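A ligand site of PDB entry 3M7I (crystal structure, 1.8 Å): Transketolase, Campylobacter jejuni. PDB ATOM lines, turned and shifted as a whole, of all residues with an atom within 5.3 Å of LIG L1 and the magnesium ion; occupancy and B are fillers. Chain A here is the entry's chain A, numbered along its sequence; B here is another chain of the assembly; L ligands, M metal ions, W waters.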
ATOM      1  N   GLY A  33       6.471 -12.134 -29.378  1.00  0.00           N
ATOM      2  CA  GLY A  33       6.516 -12.116 -27.908  1.00  0.00           C
ATOM      3  C   GLY A  33       5.225 -12.461 -27.253  1.00  0.00           C
ATOM      4  O   GLY A  33       5.154 -13.306 -26.373  1.00  0.00           O
ATOM      5  N   ALA A  34       4.180 -11.743 -27.625  1.00  0.00           N
ATOM      6  CA  ALA A  34       2.860 -11.978 -27.047  1.00  0.00           C
ATOM      7  C   ALA A  34       2.316 -13.393 -27.343  1.00  0.00           C
ATOM      8  O   ALA A  34       1.833 -14.109 -26.406  1.00  0.00           O
ATOM      9  CB  ALA A  34       1.834 -10.849 -27.457  1.00  0.00           C
ATOM     10  N   HIS A  70      -1.902  -7.652 -32.507  1.00  0.00           N
ATOM     11  CA  HIS A  70      -0.574  -7.980 -32.913  1.00  0.00           C
ATOM     12  C   HIS A  70      -0.227  -9.402 -32.578  1.00  0.00           C
ATOM     13  O   HIS A  70       0.771  -9.906 -33.107  1.00  0.00           O
ATOM     14  CB  HIS A  70       0.521  -7.019 -32.338  1.00  0.00           C
ATOM     15  CG  HIS A  70       0.581  -6.985 -30.830  1.00  0.00           C
ATOM     16  ND1 HIS A  70      -0.401  -6.362 -30.075  1.00  0.00           N
ATOM     17  CD2 HIS A  70       1.459  -7.526 -29.950  1.00  0.00           C
ATOM     18  CE1 HIS A  70      -0.125  -6.538 -28.779  1.00  0.00           C
ATOM     19  NE2 HIS A  70       1.018  -7.205 -28.678  1.00  0.00           N
ATOM     20  N   GLY A 117      -6.348  -4.631 -33.656  1.00  0.00           N
ATOM     21  CA  GLY A 117      -5.184  -3.886 -34.104  1.00  0.00           C
ATOM     22  C   GLY A 117      -5.055  -2.531 -33.415  1.00  0.00           C
ATOM     23  O   GLY A 117      -4.042  -2.256 -32.787  1.00  0.00           O
ATOM     24  N   PRO A 118      -6.050  -1.675 -33.544  1.00  0.00           N
ATOM     25  CA  PRO A 118      -5.974  -0.453 -32.734  1.00  0.00           C
ATOM     26  C   PRO A 118      -6.254  -0.839 -31.270  1.00  0.00           C
ATOM     27  O   PRO A 118      -7.310  -1.379 -30.993  1.00  0.00           O
ATOM     28  CB  PRO A 118      -7.089   0.442 -33.315  1.00  0.00           C
ATOM     29  CG  PRO A 118      -7.354  -0.198 -34.694  1.00  0.00           C
ATOM     30  CD  PRO A 118      -7.214  -1.675 -34.429  1.00  0.00           C
ATOM     31  N   LEU A 119      -5.313  -0.567 -30.396  1.00  0.00           N
ATOM     32  CA  LEU A 119      -5.404  -1.013 -28.980  1.00  0.00           C
ATOM     33  C   LEU A 119      -6.550  -0.383 -28.251  1.00  0.00           C
ATOM     34  O   LEU A 119      -7.016   0.727 -28.594  1.00  0.00           O
ATOM     35  CB  LEU A 119      -4.104  -0.776 -28.244  1.00  0.00           C
ATOM     36  CG  LEU A 119      -2.859  -1.584 -28.657  1.00  0.00           C
ATOM     37  CD1 LEU A 119      -1.629  -0.857 -28.216  1.00  0.00           C
ATOM     38  CD2 LEU A 119      -2.869  -3.053 -28.109  1.00  0.00           C
ATOM     39  N   GLY A 154      -3.644  -6.795 -23.378  1.00  0.00           N
ATOM     40  CA  GLY A 154      -2.310  -6.550 -22.885  1.00  0.00           C
ATOM     41  C   GLY A 154      -2.224  -5.225 -22.153  1.00  0.00           C
ATOM     42  O   GLY A 154      -3.246  -4.556 -21.999  1.00  0.00           O
ATOM     43  N   ASP A 155      -1.030  -4.829 -21.793  1.00  0.00           N
ATOM     44  CA  ASP A 155      -0.783  -3.553 -21.126  1.00  0.00           C
ATOM     45  C   ASP A 155      -1.328  -2.393 -21.940  1.00  0.00           C
ATOM     46  O   ASP A 155      -1.879  -1.418 -21.413  1.00  0.00           O
ATOM     47  CB  ASP A 155       0.696  -3.357 -20.889  1.00  0.00           C
ATOM     48  CG  ASP A 155       1.270  -4.442 -19.972  1.00  0.00           C
ATOM     49  OD1 ASP A 155       0.788  -4.521 -18.828  1.00  0.00           O
ATOM     50  OD2 ASP A 155       2.123  -5.221 -20.389  1.00  0.00           O
ATOM     51  N   GLY A 156      -1.143  -2.516 -23.240  1.00  0.00           N
ATOM     52  CA  GLY A 156      -1.493  -1.389 -24.091  1.00  0.00           C
ATOM     53  C   GLY A 156      -2.968  -1.157 -24.082  1.00  0.00           C
ATOM     54  O   GLY A 156      -3.445   0.001 -24.139  1.00  0.00           O
ATOM     55  N   ASP A 157      -3.727  -2.248 -24.125  1.00  0.00           N
ATOM     56  CA  ASP A 157      -5.167  -2.091 -24.165  1.00  0.00           C
ATOM     57  C   ASP A 157      -5.669  -1.367 -22.900  1.00  0.00           C
ATOM     58  O   ASP A 157      -6.603  -0.562 -22.921  1.00  0.00           O
ATOM     59  CB  ASP A 157      -5.886  -3.437 -24.240  1.00  0.00           C
ATOM     60  CG  ASP A 157      -5.561  -4.194 -25.504  1.00  0.00           C
ATOM     61  OD1 ASP A 157      -6.092  -3.750 -26.555  1.00  0.00           O
ATOM     62  OD2 ASP A 157      -4.818  -5.222 -25.403  1.00  0.00           O
ATOM     63  N   GLU A 160      -5.335   2.479 -22.636  1.00  0.00           N
ATOM     64  CA  GLU A 160      -6.228   3.311 -23.503  1.00  0.00           C
ATOM     65  C   GLU A 160      -7.504   3.667 -22.734  1.00  0.00           C
ATOM     66  O   GLU A 160      -8.156   2.801 -22.096  1.00  0.00           O
ATOM     67  CB  GLU A 160      -6.589   2.512 -24.758  1.00  0.00           C
ATOM     68  CG  GLU A 160      -5.416   2.443 -25.726  1.00  0.00           C
ATOM     69  CD  GLU A 160      -5.199   3.774 -26.469  1.00  0.00           C
ATOM     70  OE1 GLU A 160      -5.906   4.784 -26.193  1.00  0.00           O
ATOM     71  OE2 GLU A 160      -4.270   3.841 -27.306  1.00  0.00           O
ATOM     72  N   ASP A 183      -2.948 -10.105 -20.031  1.00  0.00           N
ATOM     73  CA  ASP A 183      -1.574 -10.538 -20.178  1.00  0.00           C
ATOM     74  C   ASP A 183      -0.610  -9.536 -19.531  1.00  0.00           C
ATOM     75  O   ASP A 183      -0.098  -8.641 -20.178  1.00  0.00           O
ATOM     76  CB  ASP A 183      -1.253 -10.663 -21.684  1.00  0.00           C
ATOM     77  CG  ASP A 183       0.042 -11.356 -21.938  1.00  0.00           C
ATOM     78  OD1 ASP A 183       0.505 -12.045 -21.010  1.00  0.00           O
ATOM     79  OD2 ASP A 183       0.591 -11.236 -23.079  1.00  0.00           O
ATOM     80  N   ASN A 185       2.684  -8.843 -18.578  1.00  0.00           N
ATOM     81  CA  ASN A 185       4.090  -9.225 -18.791  1.00  0.00           C
ATOM     82  C   ASN A 185       5.134  -8.119 -18.492  1.00  0.00           C
ATOM     83  O   ASN A 185       6.352  -8.296 -18.668  1.00  0.00           O
ATOM     84  CB  ASN A 185       4.234  -9.835 -20.188  1.00  0.00           C
ATOM     85  CG  ASN A 185       3.973  -8.851 -21.309  1.00  0.00           C
ATOM     86  OD1 ASN A 185       3.865  -7.614 -21.088  1.00  0.00           O
ATOM     87  ND2 ASN A 185       3.826  -9.399 -22.527  1.00  0.00           N
ATOM     88  N   ASN A 186       4.634  -6.976 -18.032  1.00  0.00           N
ATOM     89  CA  ASN A 186       5.426  -5.823 -17.678  1.00  0.00           C
ATOM     90  C   ASN A 186       6.320  -5.258 -18.787  1.00  0.00           C
ATOM     91  O   ASN A 186       7.232  -4.544 -18.504  1.00  0.00           O
ATOM     92  CB  ASN A 186       6.267  -6.150 -16.396  1.00  0.00           C
ATOM     93  CG  ASN A 186       6.936  -4.924 -15.799  1.00  0.00           C
ATOM     94  OD1 ASN A 186       8.171  -4.781 -15.855  1.00  0.00           O
ATOM     95  ND2 ASN A 186       6.135  -4.020 -15.219  1.00  0.00           N
ATOM     96  N   ILE A 187       5.975  -5.547 -20.053  1.00  0.00           N
ATOM     97  CA  ILE A 187       6.749  -5.098 -21.171  1.00  0.00           C
ATOM     98  C   ILE A 187       5.846  -4.493 -22.240  1.00  0.00           C
ATOM     99  O   ILE A 187       4.754  -5.065 -22.498  1.00  0.00           O
ATOM    100  CB  ILE A 187       7.496  -6.274 -21.778  1.00  0.00           C
ATOM    101  CG1 ILE A 187       8.568  -6.791 -20.796  1.00  0.00           C
ATOM    102  CG2 ILE A 187       8.082  -5.905 -23.200  1.00  0.00           C
ATOM    103  CD1 ILE A 187       9.711  -5.908 -20.615  1.00  0.00           C
ATOM    104  N   SER A 188       6.268  -3.333 -22.742  1.00  0.00           N
ATOM    105  CA  SER A 188       5.658  -2.659 -23.962  1.00  0.00           C
ATOM    106  C   SER A 188       6.781  -2.287 -24.870  1.00  0.00           C
ATOM    107  O   SER A 188       7.884  -2.730 -24.684  1.00  0.00           O
ATOM    108  CB  SER A 188       4.749  -1.453 -23.533  1.00  0.00           C
ATOM    109  OG  SER A 188       5.499  -0.356 -23.093  1.00  0.00           O
ATOM    110  N   ILE A 189       6.542  -1.469 -25.904  1.00  0.00           N
ATOM    111  CA  ILE A 189       7.576  -1.187 -26.876  1.00  0.00           C
ATOM    112  C   ILE A 189       8.740  -0.367 -26.302  1.00  0.00           C
ATOM    113  O   ILE A 189       9.918  -0.584 -26.642  1.00  0.00           O
ATOM    114  CB  ILE A 189       6.952  -0.470 -28.090  1.00  0.00           C
ATOM    115  CG1 ILE A 189       6.017  -1.418 -28.866  1.00  0.00           C
ATOM    116  CG2 ILE A 189       8.027   0.111 -28.983  1.00  0.00           C
ATOM    117  CD1 ILE A 189       5.255  -0.704 -30.036  1.00  0.00           C
ATOM    118  N   VAL A 193       6.979  -1.476 -18.393  1.00  0.00           N
ATOM    119  CA  VAL A 193       5.676  -0.826 -18.283  1.00  0.00           C
ATOM    120  C   VAL A 193       5.616   0.171 -17.095  1.00  0.00           C
ATOM    121  O   VAL A 193       4.904   1.193 -17.167  1.00  0.00           O
ATOM    122  CB  VAL A 193       4.610  -1.898 -18.142  1.00  0.00           C
ATOM    123  CG1 VAL A 193       3.336  -1.379 -17.547  1.00  0.00           C
ATOM    124  CG2 VAL A 193       4.332  -2.551 -19.536  1.00  0.00           C
ATOM    125  N   ILE A 245       7.018 -12.254 -21.387  1.00  0.00           N
ATOM    126  CA  ILE A 245       7.001 -12.040 -22.824  1.00  0.00           C
ATOM    127  C   ILE A 245       8.023 -12.992 -23.469  1.00  0.00           C
ATOM    128  O   ILE A 245       9.097 -13.194 -22.957  1.00  0.00           O
ATOM    129  CB  ILE A 245       7.128 -10.593 -23.255  1.00  0.00           C
ATOM    130  CG1 ILE A 245       6.714 -10.436 -24.726  1.00  0.00           C
ATOM    131  CG2 ILE A 245       8.546 -10.067 -23.149  1.00  0.00           C
ATOM    132  CD1 ILE A 245       6.843  -9.013 -25.209  1.00  0.00           C
ATOM    133  N   HIS A 259       8.961  -8.032 -28.761  1.00  0.00           N
ATOM    134  CA  HIS A 259       7.585  -7.585 -28.940  1.00  0.00           C
ATOM    135  C   HIS A 259       7.228  -7.658 -30.402  1.00  0.00           C
ATOM    136  O   HIS A 259       6.156  -8.188 -30.752  1.00  0.00           O
ATOM    137  CB  HIS A 259       7.357  -6.134 -28.454  1.00  0.00           C
ATOM    138  CG  HIS A 259       6.160  -5.490 -29.075  1.00  0.00           C
ATOM    139  ND1 HIS A 259       4.895  -5.705 -28.607  1.00  0.00           N
ATOM    140  CD2 HIS A 259       6.035  -4.695 -30.163  1.00  0.00           C
ATOM    141  CE1 HIS A 259       4.022  -5.057 -29.372  1.00  0.00           C
ATOM    142  NE2 HIS A 259       4.691  -4.443 -30.330  1.00  0.00           N
ATOM    143  N   ALA B 366       3.616   8.025 -27.534  1.00  0.00           N
ATOM    144  CA  ALA B 366       2.694   7.168 -26.877  1.00  0.00           C
ATOM    145  C   ALA B 366       3.136   5.676 -27.008  1.00  0.00           C
ATOM    146  O   ALA B 366       2.542   4.898 -27.770  1.00  0.00           O
ATOM    147  CB  ALA B 366       1.265   7.371 -27.392  1.00  0.00           C
ATOM    148  N   ASP B 367       4.135   5.297 -26.187  1.00  0.00           N
ATOM    149  CA  ASP B 367       4.795   3.985 -26.213  1.00  0.00           C
ATOM    150  C   ASP B 367       5.519   3.663 -27.502  1.00  0.00           C
ATOM    151  O   ASP B 367       5.868   2.516 -27.673  1.00  0.00           O
ATOM    152  CB  ASP B 367       3.846   2.862 -25.901  1.00  0.00           C
ATOM    153  CG  ASP B 367       4.596   1.533 -25.517  1.00  0.00           C
ATOM    154  OD1 ASP B 367       5.593   1.626 -24.743  1.00  0.00           O
ATOM    155  OD2 ASP B 367       4.210   0.473 -26.058  1.00  0.00           O
ATOM    156  N   LEU B 368       5.684   4.617 -28.429  1.00  0.00           N
ATOM    157  CA  LEU B 368       6.294   4.294 -29.749  1.00  0.00           C
ATOM    158  C   LEU B 368       7.651   4.960 -30.049  1.00  0.00           C
ATOM    159  O   LEU B 368       8.129   5.038 -31.247  1.00  0.00           O
ATOM    160  CB  LEU B 368       5.287   4.584 -30.880  1.00  0.00           C
ATOM    161  CG  LEU B 368       4.138   3.605 -30.948  1.00  0.00           C
ATOM    162  CD1 LEU B 368       3.108   4.095 -31.994  1.00  0.00           C
ATOM    163  CD2 LEU B 368       4.720   2.224 -31.329  1.00  0.00           C
ATOM    164  N   ILE B 392       0.435   4.143 -23.610  1.00  0.00           N
ATOM    165  CA  ILE B 392      -0.520   3.950 -24.689  1.00  0.00           C
ATOM    166  C   ILE B 392      -1.777   4.836 -24.449  1.00  0.00           C
ATOM    167  O   ILE B 392      -2.877   4.349 -24.204  1.00  0.00           O
ATOM    168  CB  ILE B 392      -0.858   2.484 -24.977  1.00  0.00           C
ATOM    169  CG1 ILE B 392       0.461   1.669 -25.203  1.00  0.00           C
ATOM    170  CG2 ILE B 392      -1.696   2.440 -26.281  1.00  0.00           C
ATOM    171  CD1 ILE B 392       1.216   1.173 -24.037  1.00  0.00           C
ATOM    172  N   GLU B 394      -2.701   8.185 -26.367  1.00  0.00           N
ATOM    173  CA  GLU B 394      -2.488   9.220 -27.360  1.00  0.00           C
ATOM    174  C   GLU B 394      -3.296  10.462 -27.016  1.00  0.00           C
ATOM    175  O   GLU B 394      -2.788  11.563 -27.083  1.00  0.00           O
ATOM    176  CB  GLU B 394      -3.007   8.773 -28.726  1.00  0.00           C
ATOM    177  CG  GLU B 394      -2.217   7.683 -29.354  1.00  0.00           C
ATOM    178  CD  GLU B 394      -2.615   6.303 -28.882  1.00  0.00           C
ATOM    179  OE1 GLU B 394      -3.644   6.124 -28.191  1.00  0.00           O
ATOM    180  OE2 GLU B 394      -1.865   5.349 -29.244  1.00  0.00           O
ATOM    181  N   THR B 416       3.064   9.680 -32.319  1.00  0.00           N
ATOM    182  CA  THR B 416       2.462   8.381 -32.549  1.00  0.00           C
ATOM    183  C   THR B 416       2.495   8.048 -34.086  1.00  0.00           C
ATOM    184  O   THR B 416       2.998   8.871 -34.855  1.00  0.00           O
ATOM    185  CB  THR B 416       1.039   8.270 -31.965  1.00  0.00           C
ATOM    186  OG1 THR B 416       0.595   6.926 -32.034  1.00  0.00           O
ATOM    187  CG2 THR B 416       0.067   9.337 -32.613  1.00  0.00           C
ATOM    188  N   PHE B 417       1.963   6.871 -34.443  1.00  0.00           N
ATOM    189  CA  PHE B 417       1.736   6.498 -35.861  1.00  0.00           C
ATOM    190  C   PHE B 417       0.615   7.400 -36.397  1.00  0.00           C
ATOM    191  O   PHE B 417      -0.340   7.763 -35.686  1.00  0.00           O
ATOM    192  CB  PHE B 417       1.317   5.065 -36.081  1.00  0.00           C
ATOM    193  CG  PHE B 417       2.344   4.027 -35.712  1.00  0.00           C
ATOM    194  CD1 PHE B 417       3.701   4.318 -35.789  1.00  0.00           C
ATOM    195  CD2 PHE B 417       1.932   2.805 -35.340  1.00  0.00           C
ATOM    196  CE1 PHE B 417       4.618   3.314 -35.458  1.00  0.00           C
ATOM    197  CE2 PHE B 417       2.889   1.788 -34.993  1.00  0.00           C
ATOM    198  CZ  PHE B 417       4.183   2.080 -35.101  1.00  0.00           C
ATOM    199  N   PHE B 420      -2.917   6.498 -35.684  1.00  0.00           N
ATOM    200  CA  PHE B 420      -3.444   6.756 -34.347  1.00  0.00           C
ATOM    201  C   PHE B 420      -3.482   8.249 -33.978  1.00  0.00           C
ATOM    202  O   PHE B 420      -3.840   8.583 -32.841  1.00  0.00           O
ATOM    203  CB  PHE B 420      -2.699   5.876 -33.336  1.00  0.00           C
ATOM    204  CG  PHE B 420      -2.717   4.411 -33.694  1.00  0.00           C
ATOM    205  CD1 PHE B 420      -3.843   3.793 -34.043  1.00  0.00           C
ATOM    206  CD2 PHE B 420      -1.552   3.663 -33.677  1.00  0.00           C
ATOM    207  CE1 PHE B 420      -3.885   2.383 -34.422  1.00  0.00           C
ATOM    208  CE2 PHE B 420      -1.566   2.296 -34.041  1.00  0.00           C
ATOM    209  CZ  PHE B 420      -2.733   1.686 -34.419  1.00  0.00           C
ATOM    210  N   TYR B 423      -6.929   8.939 -32.550  1.00  0.00           N
ATOM    211  CA  TYR B 423      -7.218   8.846 -31.115  1.00  0.00           C
ATOM    212  C   TYR B 423      -7.036  10.198 -30.386  1.00  0.00           C
ATOM    213  O   TYR B 423      -7.579  10.341 -29.285  1.00  0.00           O
ATOM    214  CB  TYR B 423      -6.343   7.787 -30.441  1.00  0.00           C
ATOM    215  CG  TYR B 423      -6.759   6.365 -30.518  1.00  0.00           C
ATOM    216  CD1 TYR B 423      -6.771   5.636 -31.722  1.00  0.00           C
ATOM    217  CD2 TYR B 423      -6.993   5.632 -29.336  1.00  0.00           C
ATOM    218  CE1 TYR B 423      -7.166   4.341 -31.773  1.00  0.00           C
ATOM    219  CE2 TYR B 423      -7.380   4.327 -29.392  1.00  0.00           C
ATOM    220  CZ  TYR B 423      -7.391   3.658 -30.583  1.00  0.00           C
ATOM    221  OH  TYR B 423      -7.726   2.340 -30.602  1.00  0.00           O
ATOM    222  N   HIS B 456      -3.415  -0.323 -39.798  1.00  0.00           N
ATOM    223  CA  HIS B 456      -2.259   0.487 -39.570  1.00  0.00           C
ATOM    224  C   HIS B 456      -1.833   1.354 -40.769  1.00  0.00           C
ATOM    225  O   HIS B 456      -0.780   1.962 -40.679  1.00  0.00           O
ATOM    226  CB  HIS B 456      -1.072  -0.399 -39.135  1.00  0.00           C
ATOM    227  CG  HIS B 456      -1.205  -0.928 -37.708  1.00  0.00           C
ATOM    228  ND1 HIS B 456      -0.208  -0.796 -36.748  1.00  0.00           N
ATOM    229  CD2 HIS B 456      -2.198  -1.615 -37.123  1.00  0.00           C
ATOM    230  CE1 HIS B 456      -0.632  -1.357 -35.615  1.00  0.00           C
ATOM    231  NE2 HIS B 456      -1.823  -1.877 -35.819  1.00  0.00           N
HETATM  232  N1  LIG L   1      -1.776   2.802 -30.268  1.00  0.00           N
HETATM  233  C1  LIG L   1      -2.883   2.124 -30.522  1.00  0.00           C
HETATM  234  C2  LIG L   1      -4.256   2.697 -30.258  1.00  0.00           C
HETATM  235  N2  LIG L   1      -2.775   0.944 -31.128  1.00  0.00           N
HETATM  236  C3  LIG L   1      -1.617   0.397 -31.474  1.00  0.00           C
HETATM  237  N3  LIG L   1      -1.642  -0.797 -32.061  1.00  0.00           N
HETATM  238  C4  LIG L   1      -0.378   1.094 -31.130  1.00  0.00           C
HETATM  239  C5  LIG L   1      -0.562   2.315 -30.539  1.00  0.00           C
HETATM  240  C6  LIG L   1       0.998   0.577 -31.458  1.00  0.00           C
HETATM  241  N4  LIG L   1       1.291  -0.612 -30.703  1.00  0.00           N
HETATM  242  C7  LIG L   1       1.228  -1.870 -31.132  1.00  0.00           C
HETATM  243  S1  LIG L   1       1.505  -3.078 -29.882  1.00  0.00           S
HETATM  244  C8  LIG L   1       1.851  -1.760 -28.795  1.00  0.00           C
HETATM  245  C9  LIG L   1       1.629  -0.519 -29.403  1.00  0.00           C
HETATM  246  C10 LIG L   1       1.833   0.747 -28.600  1.00  0.00           C
HETATM  247  C11 LIG L   1       2.265  -1.900 -27.371  1.00  0.00           C
HETATM  248  C12 LIG L   1       2.183  -3.309 -26.948  1.00  0.00           C
HETATM  249  O1  LIG L   1       2.143  -3.278 -25.557  1.00  0.00           O
HETATM  250  P1  LIG L   1       1.485  -4.525 -24.912  1.00  0.00           P
HETATM  251  O2  LIG L   1      -0.002  -4.502 -25.034  1.00  0.00           O
HETATM  252  O3  LIG L   1       2.014  -4.489 -23.520  1.00  0.00           O
HETATM  253  O4  LIG L   1       1.946  -5.759 -25.834  1.00  0.00           O
HETATM  254  P2  LIG L   1       3.176  -6.753 -25.537  1.00  0.00           P
HETATM  255  O5  LIG L   1       3.181  -7.635 -26.745  1.00  0.00           O
HETATM  256  O6  LIG L   1       2.942  -7.330 -24.136  1.00  0.00           O
HETATM  257  O7  LIG L   1       4.415  -5.916 -25.600  1.00  0.00           O
HETATM  258  C1  LG2 L   2       3.506  -2.443 -34.395  1.00  0.00           C
HETATM  259  O1  LG2 L   2       4.310  -1.428 -34.927  1.00  0.00           O
HETATM  260  C2  LG2 L   2       4.436  -3.295 -33.548  1.00  0.00           C
HETATM  261  O2  LG2 L   2       4.149  -2.998 -32.201  1.00  0.00           O
HETATM  262  C3  LG2 L   2       5.841  -3.008 -34.045  1.00  0.00           C
HETATM  263  O3  LG2 L   2       6.829  -2.888 -33.047  1.00  0.00           O
HETATM  264  C4  LG2 L   2       5.668  -1.677 -34.716  1.00  0.00           C
HETATM  265  C5  LG2 L   2       6.332  -1.697 -36.062  1.00  0.00           C
HETATM  266  O4  LG2 L   2       7.731  -1.566 -35.816  1.00  0.00           O
HETATM  267  P1  LG2 L   2       8.472  -0.738 -36.919  1.00  0.00           P
HETATM  268  O5  LG2 L   2       9.296   0.395 -36.381  1.00  0.00           O
HETATM  269  O6  LG2 L   2       7.257  -0.289 -37.912  1.00  0.00           O
HETATM  270  O7  LG2 L   2       9.579  -1.600 -37.703  1.00  0.00           O
HETATM  271  O8  LG2 L   2       2.998  -3.251 -35.437  1.00  0.00           O
HETATM  272 MG    MG M   1       2.851  -6.079 -22.275  1.00  0.00          MG
HETATM  273  O   HOH W   1      -0.276  -3.607 -33.380  1.00  0.00           O
HETATM  274  O   HOH W   2       4.348  -9.043 -28.825  1.00  0.00           O
HETATM  275  O   HOH W   3       0.656   5.361 -29.984  1.00  0.00           O
HETATM  276  O   HOH W   4      -2.013  -5.894 -26.245  1.00  0.00           O
HETATM  277  O   HOH W   5       0.494  -9.034 -24.354  1.00  0.00           O
HETATM  278  O   HOH W   6       1.035  -7.149 -22.267  1.00  0.00           O
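A sulfur (S1) of LIG L1 sits close to an oxygen (O2) of LG2 L2, at 3.5 Å.
Of the 30 residues printed, 3 come within 4 Å of the magnesium ion.
CB of Ala 34 touches O5 of LIG L1 (3.6 Å).
Pro 118 touches LIG L1 (CA to N2, 3.8 Å).
C of Gly 154 touches O2 of LIG L1 (3.7 Å).
OE2 of Glu 160 touches C2 of LIG L1 (3.2 Å).
CB of Ser 188 touches O1 of LIG L1 (3.8 Å).
Ile 189 touches LIG L1.
CD1 of Ile 245 touches O7 of LIG L1 (3.95 Å).
OD2 of Asp 367 of chain B touches C11 of LIG L1, at 3.3 Å.
Ile 392 of chain B touches LIG L1.
Phe 420 of chain B touches LIG L1.
CZ of Tyr 423 of chain B touches C2 of LIG L1, at 3.3 Å.
CE1 of His 456 of chain B touches N3 of LIG L1, at 3.7 Å.
Hydrophobic or aromatic side chains that line LIG L1: Ala 34, His 70, Leu 119, Ile 189, Ile 245, His 259, Ile 392 of chain B, Phe 420 of chain B, Tyr 423 of chain B and His 456 of chain B.
Within 4 Å of LIG L1: Ala 34, His 70, Gly 117, Pro 118, Leu 119, Gly 154, Asp 155, Gly 156, Glu 160, Asn 185, Ile 187, Ser 188, Ile 189, Ile 245, His 259, Asp 367 of chain B, Ile 392 of chain B, Glu 394 of chain B, Phe 420 of chain B, Tyr 423 of chain B and His 456 of chain B.
The nearest printed residue that does not touch LIG L1 is Leu 368 of chain B (4.1 Å).
Water W6 bridges the backbone carbonyl oxygen of Asp 183 (2.8 Å) and the backbone NH of Asp 155 (3.1 Å).
Water W4 lies within hydrogen-bond range of O2 of LIG L1, OD2 of Asp 157 and N of Gly 154.
Water W2 lies within hydrogen-bond range of an oxygen (O5) of LIG L1, the backbone carbonyl oxygen of His 259 and the backbone NH of Ala 34.
Water W1 lies within hydrogen-bond range of a ring nitrogen (NE2) of His 456 of chain B (3.4 Å) and a nitrogen (N3) of LIG L1 (3.4 Å).
Water W3 lies within hydrogen-bond range of the side-chain hydroxyl of Thr 416 of chain B (2.6 Å), the side-chain carboxylate of Glu 394 of chain B (2.6 Å) and the backbone carbonyl oxygen of Ala 366 of chain B (2.9 Å).
The magnesium ion is bound by water W6 (2.1 Å), O of Ile 187 (2.2 Å), O3 of LIG L1 (2.2 Å), OD1 of Asn 185 (2.2 Å), OD2 of Asp 155 (2.2 Å) and O6 of LIG L1 (2.2 Å).
The side-chain carboxylate (OE1) of Glu 394 of chain B lies close to the side-chain carboxylate (OE2) of Glu 160, at 2.5 Å.
OH of Tyr 423 of chain B is in hydrogen-bond range of O of Leu 119, at 2.7 Å.
The backbone carbonyl oxygen (O) of Ile 392 of chain B lies close to the backbone NH (N) of Glu 160, at 3.5 Å.
The backbone NH (N) of Ile 189 sits at hydrogen-bond distance from the side-chain carboxylate (OD2) of Asp 367 of chain B, 3.0 Å away.
The side-chain carboxylate of Asp 367 of chain B lies within hydrogen-bond range of the side-chain hydroxyl of Ser 188 (2.6 Å).
N of Gly 154 sits at hydrogen-bond distance from OD2 of Asp 157.
An oxygen (O2) of LIG L1 lies within hydrogen-bond range of the backbone NH of Asp 155 (3.4 Å).
A nitrogen (N1) of LIG L1 sits at hydrogen-bond distance from the side-chain carboxylate (OE2) of Glu 394 of chain B (2.7 Å).
O of Gly 117 is in hydrogen-bond range of N3 of LIG L1.
An oxygen (O2) of LIG L1 is in hydrogen-bond range of the backbone NH (N) of Gly 156 (2.9 Å).
An oxygen (O5) of LIG L1 is in hydrogen-bond range of a ring nitrogen (NE2) of His 70 (2.9 Å).
N of Leu 119 sits at hydrogen-bond distance from N2 of LIG L1 (3.0 Å).
A ring nitrogen (ND1) of His 259 lies within hydrogen-bond range of an oxygen (O7) of LIG L1 (3.1 Å).
An oxygen (O2) of LG2 L2 lies within hydrogen-bond range of a ring nitrogen (NE2) of His 259.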
